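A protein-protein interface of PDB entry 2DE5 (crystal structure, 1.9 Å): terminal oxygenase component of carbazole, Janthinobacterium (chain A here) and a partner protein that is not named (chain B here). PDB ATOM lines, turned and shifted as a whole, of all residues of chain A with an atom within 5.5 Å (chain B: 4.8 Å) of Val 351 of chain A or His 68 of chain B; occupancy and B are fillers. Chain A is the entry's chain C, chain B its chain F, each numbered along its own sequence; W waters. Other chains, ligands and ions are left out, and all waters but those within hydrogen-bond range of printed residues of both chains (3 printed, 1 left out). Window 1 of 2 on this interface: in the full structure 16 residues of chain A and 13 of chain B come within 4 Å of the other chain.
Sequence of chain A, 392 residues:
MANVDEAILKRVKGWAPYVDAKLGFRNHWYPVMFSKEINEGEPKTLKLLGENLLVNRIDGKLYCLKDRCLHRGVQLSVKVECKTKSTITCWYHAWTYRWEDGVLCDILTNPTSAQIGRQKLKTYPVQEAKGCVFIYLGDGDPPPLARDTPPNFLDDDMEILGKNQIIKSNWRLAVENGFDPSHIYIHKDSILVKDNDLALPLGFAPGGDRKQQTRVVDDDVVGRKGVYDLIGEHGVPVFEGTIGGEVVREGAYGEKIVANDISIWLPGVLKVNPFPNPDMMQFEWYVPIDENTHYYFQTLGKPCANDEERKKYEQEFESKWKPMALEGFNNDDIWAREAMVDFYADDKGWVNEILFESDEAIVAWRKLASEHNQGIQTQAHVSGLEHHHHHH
The guanidinium group of Arg 11 of chain A sits at hydrogen-bond distance from the backbone carbonyl oxygen of His 68 of chain B, 2.9 Å away. The backbone NH of Gly 69 of chain B lies within hydrogen-bond range of the backbone carbonyl oxygen of Arg 11 of chain A, 3.3 Å away. O of Asn 352 of chain A is in hydrogen-bond range of NE2 of His 48 of chain B. O of Glu 353 of chain A sits close to NE2 of His 48 of chain B (3.3 Å). NE2 of His 68 of chain B sits at hydrogen-bond distance from OE2 of Glu 353 of chain A. O of Phe 67 of chain B sits close to O of Arg 11 of chain A, at 3.5 Å.
The backbone carbonyl oxygen (O) of Lys 348 of chain A is in hydrogen-bond range of the side-chain amide nitrogen (ND2) of Asn 352 of chain A, at 3.2 Å. The side-chain carboxylate (OE2) of Glu 353 of chain A lies within salt-bridge range of the guanidinium group (NH1) of Arg 366 of chain A, at 2.7 Å. The side-chain sulfur (SG) of Cys 65 of chain B lies close to the backbone NH (N) of Phe 67 of chain B, at 3.5 Å. The backbone carbonyl oxygen (O) of Gly 70 of chain B is in hydrogen-bond range of the backbone NH (N) of Cys 65 of chain B (2.7 Å).
Among the printed residues, merely in contact across the chains: Trp 350 of chain A with His 68 of chain B (3.0 Å), Val 351 of chain A with His 68 of chain B (3.2 Å), Val 351 of chain A with His 48 of chain B (3.3 Å), Val 351 of chain A with Pro 83 of chain B (3.3 Å), Val 12 of chain A with Phe 67 of chain B (3.5 Å), Asn 352 of chain A with Pro 83 of chain B (3.5 Å), Arg 11 of chain A with Pro 83 of chain B (3.6 Å), Trp 15 of chain A with Phe 67 of chain B (3.6 Å), Arg 11 of chain A with Gly 70 of chain B (3.95 Å) and Leu 355 of chain A with Phe 67 of chain B (3.99 Å).
Of the printed residues of chain B, Arg 11 of chain A touches Phe 67 (3.5 Å), His 68 (2.9 Å), Gly 69 (3.3 Å), Gly 70 (3.95 Å) and Pro 83 (3.6 Å). Val 351 of chain A touches three residues of chain B. Of the printed residues of chain B, Glu 353 of chain A touches His 48 (2.9 Å) and His 68 (2.9 Å). Printed residues of chain A within 4 Å of His 48 of chain B: Val 351, Asn 352 and Glu 353. His 68 of chain B touches just these residues of chain A: Arg 11 (2.9 Å), Trp 350 (3.0 Å), Val 351 (3.2 Å) and Glu 353 (2.9 Å). The nearest printed residue of chain B that does not touch Val 351 of chain A is Gly 69 of chain B (5.9 Å). The nearest printed residue of chain B that does not touch Val 12 of chain A is His 68 of chain B (4.6 Å).
Of the 8 printed residues of chain B, 6 touch a printed residue of chain A. Hydrophobic or aromatic side chains of chain B that line the printed part of chain A: His 48, Phe 67, His 68 and Pro 83. Printed residues of chain A that touch a printed residue of chain B: Arg 11, Val 12, Trp 15, Trp 350, Val 351, Asn 352, Glu 353 and Leu 355. Among the printed residues, 16 pairs touch across the chains. Among the printed residues, no Asp or Glu carboxylate lies within 4 Å of a Lys or Arg side-chain nitrogen of the other chain.
Water W2 lies within hydrogen-bond range of the backbone carbonyl oxygen of His 48 of chain B (2.7 Å), the backbone carbonyl oxygen of Glu 353 of chain A (2.8 Å) and the backbone NH of Leu 355 of chain A (2.8 Å). Water W3 lies within hydrogen-bond range of the backbone carbonyl oxygen (O) of Arg 11 of chain A (2.8 Å), the backbone carbonyl oxygen (O) of Cys 65 of chain B (2.9 Å) and the backbone NH (N) of Gly 69 of chain B (3.3 Å). Water W1 bridges a ring nitrogen (NE2) of His 48 of chain B (3.0 Å) and the backbone carbonyl oxygen of Asn 352 of chain A (3.2 Å).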
ATOM      1  N   ILE A   8      -6.482 -25.870  28.835  1.00  0.00           N
ATOM      2  CA  ILE A   8      -5.372 -25.422  28.005  1.00  0.00           C
ATOM      3  C   ILE A   8      -5.143 -26.403  26.861  1.00  0.00           C
ATOM      4  O   ILE A   8      -4.951 -26.001  25.717  1.00  0.00           O
ATOM      5  CB  ILE A   8      -4.065 -25.288  28.830  1.00  0.00           C
ATOM      6  CG1 ILE A   8      -4.218 -24.171  29.863  1.00  0.00           C
ATOM      7  CG2 ILE A   8      -2.887 -24.992  27.907  1.00  0.00           C
ATOM      8  CD1 ILE A   8      -3.005 -23.983  30.754  1.00  0.00           C
ATOM      9  N   ARG A  11      -7.307 -25.958  23.984  1.00  0.00           N
ATOM     10  CA  ARG A  11      -6.993 -24.784  23.171  1.00  0.00           C
ATOM     11  C   ARG A  11      -5.907 -25.032  22.127  1.00  0.00           C
ATOM     12  O   ARG A  11      -5.942 -24.450  21.044  1.00  0.00           O
ATOM     13  CB  ARG A  11      -6.568 -23.613  24.064  1.00  0.00           C
ATOM     14  CG  ARG A  11      -7.715 -22.822  24.676  1.00  0.00           C
ATOM     15  CD  ARG A  11      -7.190 -21.754  25.648  1.00  0.00           C
ATOM     16  NE  ARG A  11      -8.191 -20.727  25.945  1.00  0.00           N
ATOM     17  CZ  ARG A  11      -8.458 -19.685  25.157  1.00  0.00           C
ATOM     18  NH1 ARG A  11      -7.798 -19.519  24.017  1.00  0.00           N
ATOM     19  NH2 ARG A  11      -9.391 -18.809  25.509  1.00  0.00           N
ATOM     20  N   VAL A  12      -4.940 -25.885  22.455  1.00  0.00           N
ATOM     21  CA  VAL A  12      -3.853 -26.183  21.529  1.00  0.00           C
ATOM     22  C   VAL A  12      -4.124 -27.471  20.755  1.00  0.00           C
ATOM     23  O   VAL A  12      -3.362 -28.428  20.836  1.00  0.00           O
ATOM     24  CB  VAL A  12      -2.504 -26.298  22.277  1.00  0.00           C
ATOM     25  CG1 VAL A  12      -2.075 -24.922  22.789  1.00  0.00           C
ATOM     26  CG2 VAL A  12      -2.631 -27.271  23.438  1.00  0.00           C
ATOM     27  N   TRP A  15      -1.303 -29.470  18.799  1.00  0.00           N
ATOM     28  CA  TRP A  15      -0.222 -30.214  19.436  1.00  0.00           C
ATOM     29  C   TRP A  15      -0.444 -30.445  20.929  1.00  0.00           C
ATOM     30  O   TRP A  15       0.457 -30.253  21.748  1.00  0.00           O
ATOM     31  CB  TRP A  15       1.108 -29.487  19.180  1.00  0.00           C
ATOM     32  CG  TRP A  15       1.071 -27.992  19.414  1.00  0.00           C
ATOM     33  CD1 TRP A  15       1.152 -27.348  20.614  1.00  0.00           C
ATOM     34  CD2 TRP A  15       0.926 -26.967  18.420  1.00  0.00           C
ATOM     35  NE1 TRP A  15       1.066 -25.985  20.432  1.00  0.00           N
ATOM     36  CE2 TRP A  15       0.926 -25.724  19.096  1.00  0.00           C
ATOM     37  CE3 TRP A  15       0.795 -26.977  17.025  1.00  0.00           C
ATOM     38  CZ2 TRP A  15       0.801 -24.499  18.423  1.00  0.00           C
ATOM     39  CZ3 TRP A  15       0.670 -25.757  16.354  1.00  0.00           C
ATOM     40  CH2 TRP A  15       0.675 -24.537  17.057  1.00  0.00           C
ATOM     41  N   ASP A 347       2.104 -23.039  32.255  1.00  0.00           N
ATOM     42  CA  ASP A 347       1.512 -23.629  31.053  1.00  0.00           C
ATOM     43  C   ASP A 347       0.752 -22.609  30.196  1.00  0.00           C
ATOM     44  O   ASP A 347       0.215 -22.963  29.147  1.00  0.00           O
ATOM     45  CB  ASP A 347       0.560 -24.779  31.413  1.00  0.00           C
ATOM     46  CG  ASP A 347       1.285 -26.003  31.963  1.00  0.00           C
ATOM     47  OD1 ASP A 347       2.290 -26.434  31.351  1.00  0.00           O
ATOM     48  OD2 ASP A 347       0.837 -26.542  33.001  1.00  0.00           O
ATOM     49  N   LYS A 348       0.719 -21.349  30.626  1.00  0.00           N
ATOM     50  CA  LYS A 348      -0.013 -20.318  29.883  1.00  0.00           C
ATOM     51  C   LYS A 348       0.698 -19.820  28.625  1.00  0.00           C
ATOM     52  O   LYS A 348       0.052 -19.332  27.700  1.00  0.00           O
ATOM     53  CB  LYS A 348      -0.332 -19.124  30.793  1.00  0.00           C
ATOM     54  CG  LYS A 348      -1.197 -19.469  32.006  1.00  0.00           C
ATOM     55  CD  LYS A 348      -2.510 -20.111  31.589  1.00  0.00           C
ATOM     56  CE  LYS A 348      -3.326 -20.565  32.801  1.00  0.00           C
ATOM     57  NZ  LYS A 348      -3.713 -19.433  33.687  1.00  0.00           N
ATOM     58  N   GLY A 349       2.023 -19.941  28.598  1.00  0.00           N
ATOM     59  CA  GLY A 349       2.785 -19.496  27.446  1.00  0.00           C
ATOM     60  C   GLY A 349       2.434 -20.272  26.189  1.00  0.00           C
ATOM     61  O   GLY A 349       2.591 -19.771  25.070  1.00  0.00           O
ATOM     62  N   TRP A 350       1.956 -21.502  26.369  1.00  0.00           N
ATOM     63  CA  TRP A 350       1.579 -22.339  25.235  1.00  0.00           C
ATOM     64  C   TRP A 350       0.357 -21.759  24.530  1.00  0.00           C
ATOM     65  O   TRP A 350       0.027 -22.155  23.418  1.00  0.00           O
ATOM     66  CB  TRP A 350       1.286 -23.775  25.695  1.00  0.00           C
ATOM     67  CG  TRP A 350       2.475 -24.474  26.293  1.00  0.00           C
ATOM     68  CD1 TRP A 350       2.647 -24.835  27.602  1.00  0.00           C
ATOM     69  CD2 TRP A 350       3.671 -24.875  25.606  1.00  0.00           C
ATOM     70  NE1 TRP A 350       3.876 -25.432  27.773  1.00  0.00           N
ATOM     71  CE2 TRP A 350       4.525 -25.469  26.565  1.00  0.00           C
ATOM     72  CE3 TRP A 350       4.103 -24.787  24.275  1.00  0.00           C
ATOM     73  CZ2 TRP A 350       5.792 -25.972  26.234  1.00  0.00           C
ATOM     74  CZ3 TRP A 350       5.361 -25.287  23.943  1.00  0.00           C
ATOM     75  CH2 TRP A 350       6.191 -25.873  24.925  1.00  0.00           C
ATOM     76  N   VAL A 351      -0.316 -20.821  25.186  1.00  0.00           N
ATOM     77  CA  VAL A 351      -1.485 -20.181  24.594  1.00  0.00           C
ATOM     78  C   VAL A 351      -1.231 -18.712  24.248  1.00  0.00           C
ATOM     79  O   VAL A 351      -1.707 -18.224  23.227  1.00  0.00           O
ATOM     80  CB  VAL A 351      -2.709 -20.245  25.548  1.00  0.00           C
ATOM     81  CG1 VAL A 351      -3.841 -19.364  25.017  1.00  0.00           C
ATOM     82  CG2 VAL A 351      -3.183 -21.675  25.686  1.00  0.00           C
ATOM     83  N   ASN A 352      -0.465 -18.021  25.088  1.00  0.00           N
ATOM     84  CA  ASN A 352      -0.208 -16.596  24.898  1.00  0.00           C
ATOM     85  C   ASN A 352       0.949 -16.167  23.995  1.00  0.00           C
ATOM     86  O   ASN A 352       1.043 -14.996  23.637  1.00  0.00           O
ATOM     87  CB  ASN A 352      -0.069 -15.932  26.266  1.00  0.00           C
ATOM     88  CG  ASN A 352      -1.345 -16.039  27.084  1.00  0.00           C
ATOM     89  OD1 ASN A 352      -2.423 -15.715  26.594  1.00  0.00           O
ATOM     90  ND2 ASN A 352      -1.231 -16.495  28.325  1.00  0.00           N
ATOM     91  N   GLU A 353       1.822 -17.102  23.637  1.00  0.00           N
ATOM     92  CA  GLU A 353       2.957 -16.806  22.754  1.00  0.00           C
ATOM     93  C   GLU A 353       2.467 -16.188  21.445  1.00  0.00           C
ATOM     94  O   GLU A 353       1.425 -16.576  20.937  1.00  0.00           O
ATOM     95  CB  GLU A 353       3.705 -18.103  22.422  1.00  0.00           C
ATOM     96  CG  GLU A 353       2.773 -19.177  21.862  1.00  0.00           C
ATOM     97  CD  GLU A 353       3.458 -20.502  21.568  1.00  0.00           C
ATOM     98  OE1 GLU A 353       4.539 -20.772  22.142  1.00  0.00           O
ATOM     99  OE2 GLU A 353       2.893 -21.282  20.768  1.00  0.00           O
ATOM    100  N   LEU A 355       3.703 -15.935  17.791  1.00  0.00           N
ATOM    101  CA  LEU A 355       4.691 -16.446  16.850  1.00  0.00           C
ATOM    102  C   LEU A 355       4.823 -15.636  15.567  1.00  0.00           C
ATOM    103  O   LEU A 355       3.913 -14.895  15.189  1.00  0.00           O
ATOM    104  CB  LEU A 355       4.329 -17.894  16.482  1.00  0.00           C
ATOM    105  CG  LEU A 355       4.080 -18.860  17.650  1.00  0.00           C
ATOM    106  CD1 LEU A 355       3.722 -20.241  17.116  1.00  0.00           C
ATOM    107  CD2 LEU A 355       5.321 -18.938  18.526  1.00  0.00           C
ATOM    108  N   ARG A 366       6.381 -29.529  16.733  1.00  0.00           N
ATOM    109  CA  ARG A 366       5.323 -29.766  17.709  1.00  0.00           C
ATOM    110  C   ARG A 366       4.308 -30.766  17.158  1.00  0.00           C
ATOM    111  O   ARG A 366       3.840 -31.647  17.878  1.00  0.00           O
ATOM    112  CB  ARG A 366       4.612 -28.460  18.063  1.00  0.00           C
ATOM    113  CG  ARG A 366       5.428 -27.504  18.920  1.00  0.00           C
ATOM    114  CD  ARG A 366       4.635 -26.238  19.232  1.00  0.00           C
ATOM    115  NE  ARG A 366       5.400 -25.269  20.016  1.00  0.00           N
ATOM    116  CZ  ARG A 366       4.997 -24.026  20.252  1.00  0.00           C
ATOM    117  NH1 ARG A 366       3.839 -23.605  19.764  1.00  0.00           N
ATOM    118  NH2 ARG A 366       5.754 -23.199  20.963  1.00  0.00           N
ATOM    119  N   HIS B  48      -3.021 -13.010  16.095  1.00  0.00           N
ATOM    120  CA  HIS B  48      -2.225 -13.359  17.270  1.00  0.00           C
ATOM    121  C   HIS B  48      -0.979 -14.173  16.928  1.00  0.00           C
ATOM    122  O   HIS B  48      -0.138 -14.423  17.793  1.00  0.00           O
ATOM    123  CB  HIS B  48      -3.096 -14.131  18.276  1.00  0.00           C
ATOM    124  CG  HIS B  48      -2.365 -14.569  19.507  1.00  0.00           C
ATOM    125  ND1 HIS B  48      -2.011 -15.882  19.731  1.00  0.00           N
ATOM    126  CD2 HIS B  48      -1.913 -13.871  20.578  1.00  0.00           C
ATOM    127  CE1 HIS B  48      -1.373 -15.976  20.884  1.00  0.00           C
ATOM    128  NE2 HIS B  48      -1.299 -14.770  21.419  1.00  0.00           N
ATOM    129  N   CYS B  65      -9.291 -20.095  16.105  1.00  0.00           N
ATOM    130  CA  CYS B  65      -7.953 -20.337  15.577  1.00  0.00           C
ATOM    131  C   CYS B  65      -7.430 -21.716  15.997  1.00  0.00           C
ATOM    132  O   CYS B  65      -7.549 -22.106  17.159  1.00  0.00           O
ATOM    133  CB  CYS B  65      -7.000 -19.251  16.072  1.00  0.00           C
ATOM    134  SG  CYS B  65      -5.314 -19.524  15.541  1.00  0.00           S
ATOM    135  N   PRO B  66      -6.822 -22.461  15.056  1.00  0.00           N
ATOM    136  CA  PRO B  66      -6.278 -23.801  15.305  1.00  0.00           C
ATOM    137  C   PRO B  66      -5.048 -23.872  16.210  1.00  0.00           C
ATOM    138  O   PRO B  66      -4.717 -24.942  16.729  1.00  0.00           O
ATOM    139  CB  PRO B  66      -5.970 -24.306  13.901  1.00  0.00           C
ATOM    140  CG  PRO B  66      -5.537 -23.061  13.203  1.00  0.00           C
ATOM    141  CD  PRO B  66      -6.596 -22.067  13.653  1.00  0.00           C
ATOM    142  N   PHE B  67      -4.375 -22.740  16.392  1.00  0.00           N
ATOM    143  CA  PHE B  67      -3.168 -22.680  17.217  1.00  0.00           C
ATOM    144  C   PHE B  67      -3.386 -22.594  18.722  1.00  0.00           C
ATOM    145  O   PHE B  67      -3.010 -23.505  19.466  1.00  0.00           O
ATOM    146  CB  PHE B  67      -2.301 -21.487  16.787  1.00  0.00           C
ATOM    147  CG  PHE B  67      -1.295 -21.809  15.714  1.00  0.00           C
ATOM    148  CD1 PHE B  67      -1.570 -22.763  14.737  1.00  0.00           C
ATOM    149  CD2 PHE B  67      -0.097 -21.101  15.640  1.00  0.00           C
ATOM    150  CE1 PHE B  67      -0.667 -23.002  13.699  1.00  0.00           C
ATOM    151  CE2 PHE B  67       0.812 -21.331  14.606  1.00  0.00           C
ATOM    152  CZ  PHE B  67       0.526 -22.281  13.633  1.00  0.00           C
ATOM    153  N   HIS B  68      -3.990 -21.498  19.173  1.00  0.00           N
ATOM    154  CA  HIS B  68      -4.194 -21.281  20.603  1.00  0.00           C
ATOM    155  C   HIS B  68      -5.644 -21.168  21.071  1.00  0.00           C
ATOM    156  O   HIS B  68      -5.903 -20.908  22.246  1.00  0.00           O
ATOM    157  CB  HIS B  68      -3.419 -20.032  21.030  1.00  0.00           C
ATOM    158  CG  HIS B  68      -1.988 -20.035  20.590  1.00  0.00           C
ATOM    159  ND1 HIS B  68      -1.495 -19.157  19.651  1.00  0.00           N
ATOM    160  CD2 HIS B  68      -0.947 -20.826  20.946  1.00  0.00           C
ATOM    161  CE1 HIS B  68      -0.213 -19.404  19.448  1.00  0.00           C
ATOM    162  NE2 HIS B  68       0.144 -20.413  20.222  1.00  0.00           N
ATOM    163  N   GLY B  69      -6.592 -21.362  20.165  1.00  0.00           N
ATOM    164  CA  GLY B  69      -7.980 -21.282  20.577  1.00  0.00           C
ATOM    165  C   GLY B  69      -8.523 -19.872  20.632  1.00  0.00           C
ATOM    166  O   GLY B  69      -9.614 -19.647  21.159  1.00  0.00           O
ATOM    167  N   GLY B  70      -7.766 -18.910  20.113  1.00  0.00           N
ATOM    168  CA  GLY B  70      -8.260 -17.547  20.088  1.00  0.00           C
ATOM    169  C   GLY B  70      -9.410 -17.593  19.100  1.00  0.00           C
ATOM    170  O   GLY B  70      -9.542 -18.578  18.372  1.00  0.00           O
ATOM    171  N   PRO B  83      -6.476 -15.708  23.230  1.00  0.00           N
ATOM    172  CA  PRO B  83      -5.621 -14.543  23.477  1.00  0.00           C
ATOM    173  C   PRO B  83      -5.666 -13.464  22.390  1.00  0.00           C
ATOM    174  O   PRO B  83      -4.902 -12.505  22.437  1.00  0.00           O
ATOM    175  CB  PRO B  83      -4.236 -15.164  23.602  1.00  0.00           C
ATOM    176  CG  PRO B  83      -4.295 -16.247  22.557  1.00  0.00           C
ATOM    177  CD  PRO B  83      -5.664 -16.866  22.806  1.00  0.00           C
HETATM  178  O   HOH W   1      -1.170 -12.727  23.579  1.00  0.00           O
HETATM  179  O   HOH W   2       1.055 -16.867  18.198  1.00  0.00           O
HETATM  180  O   HOH W   3      -8.064 -24.166  19.171  1.00  0.00           O
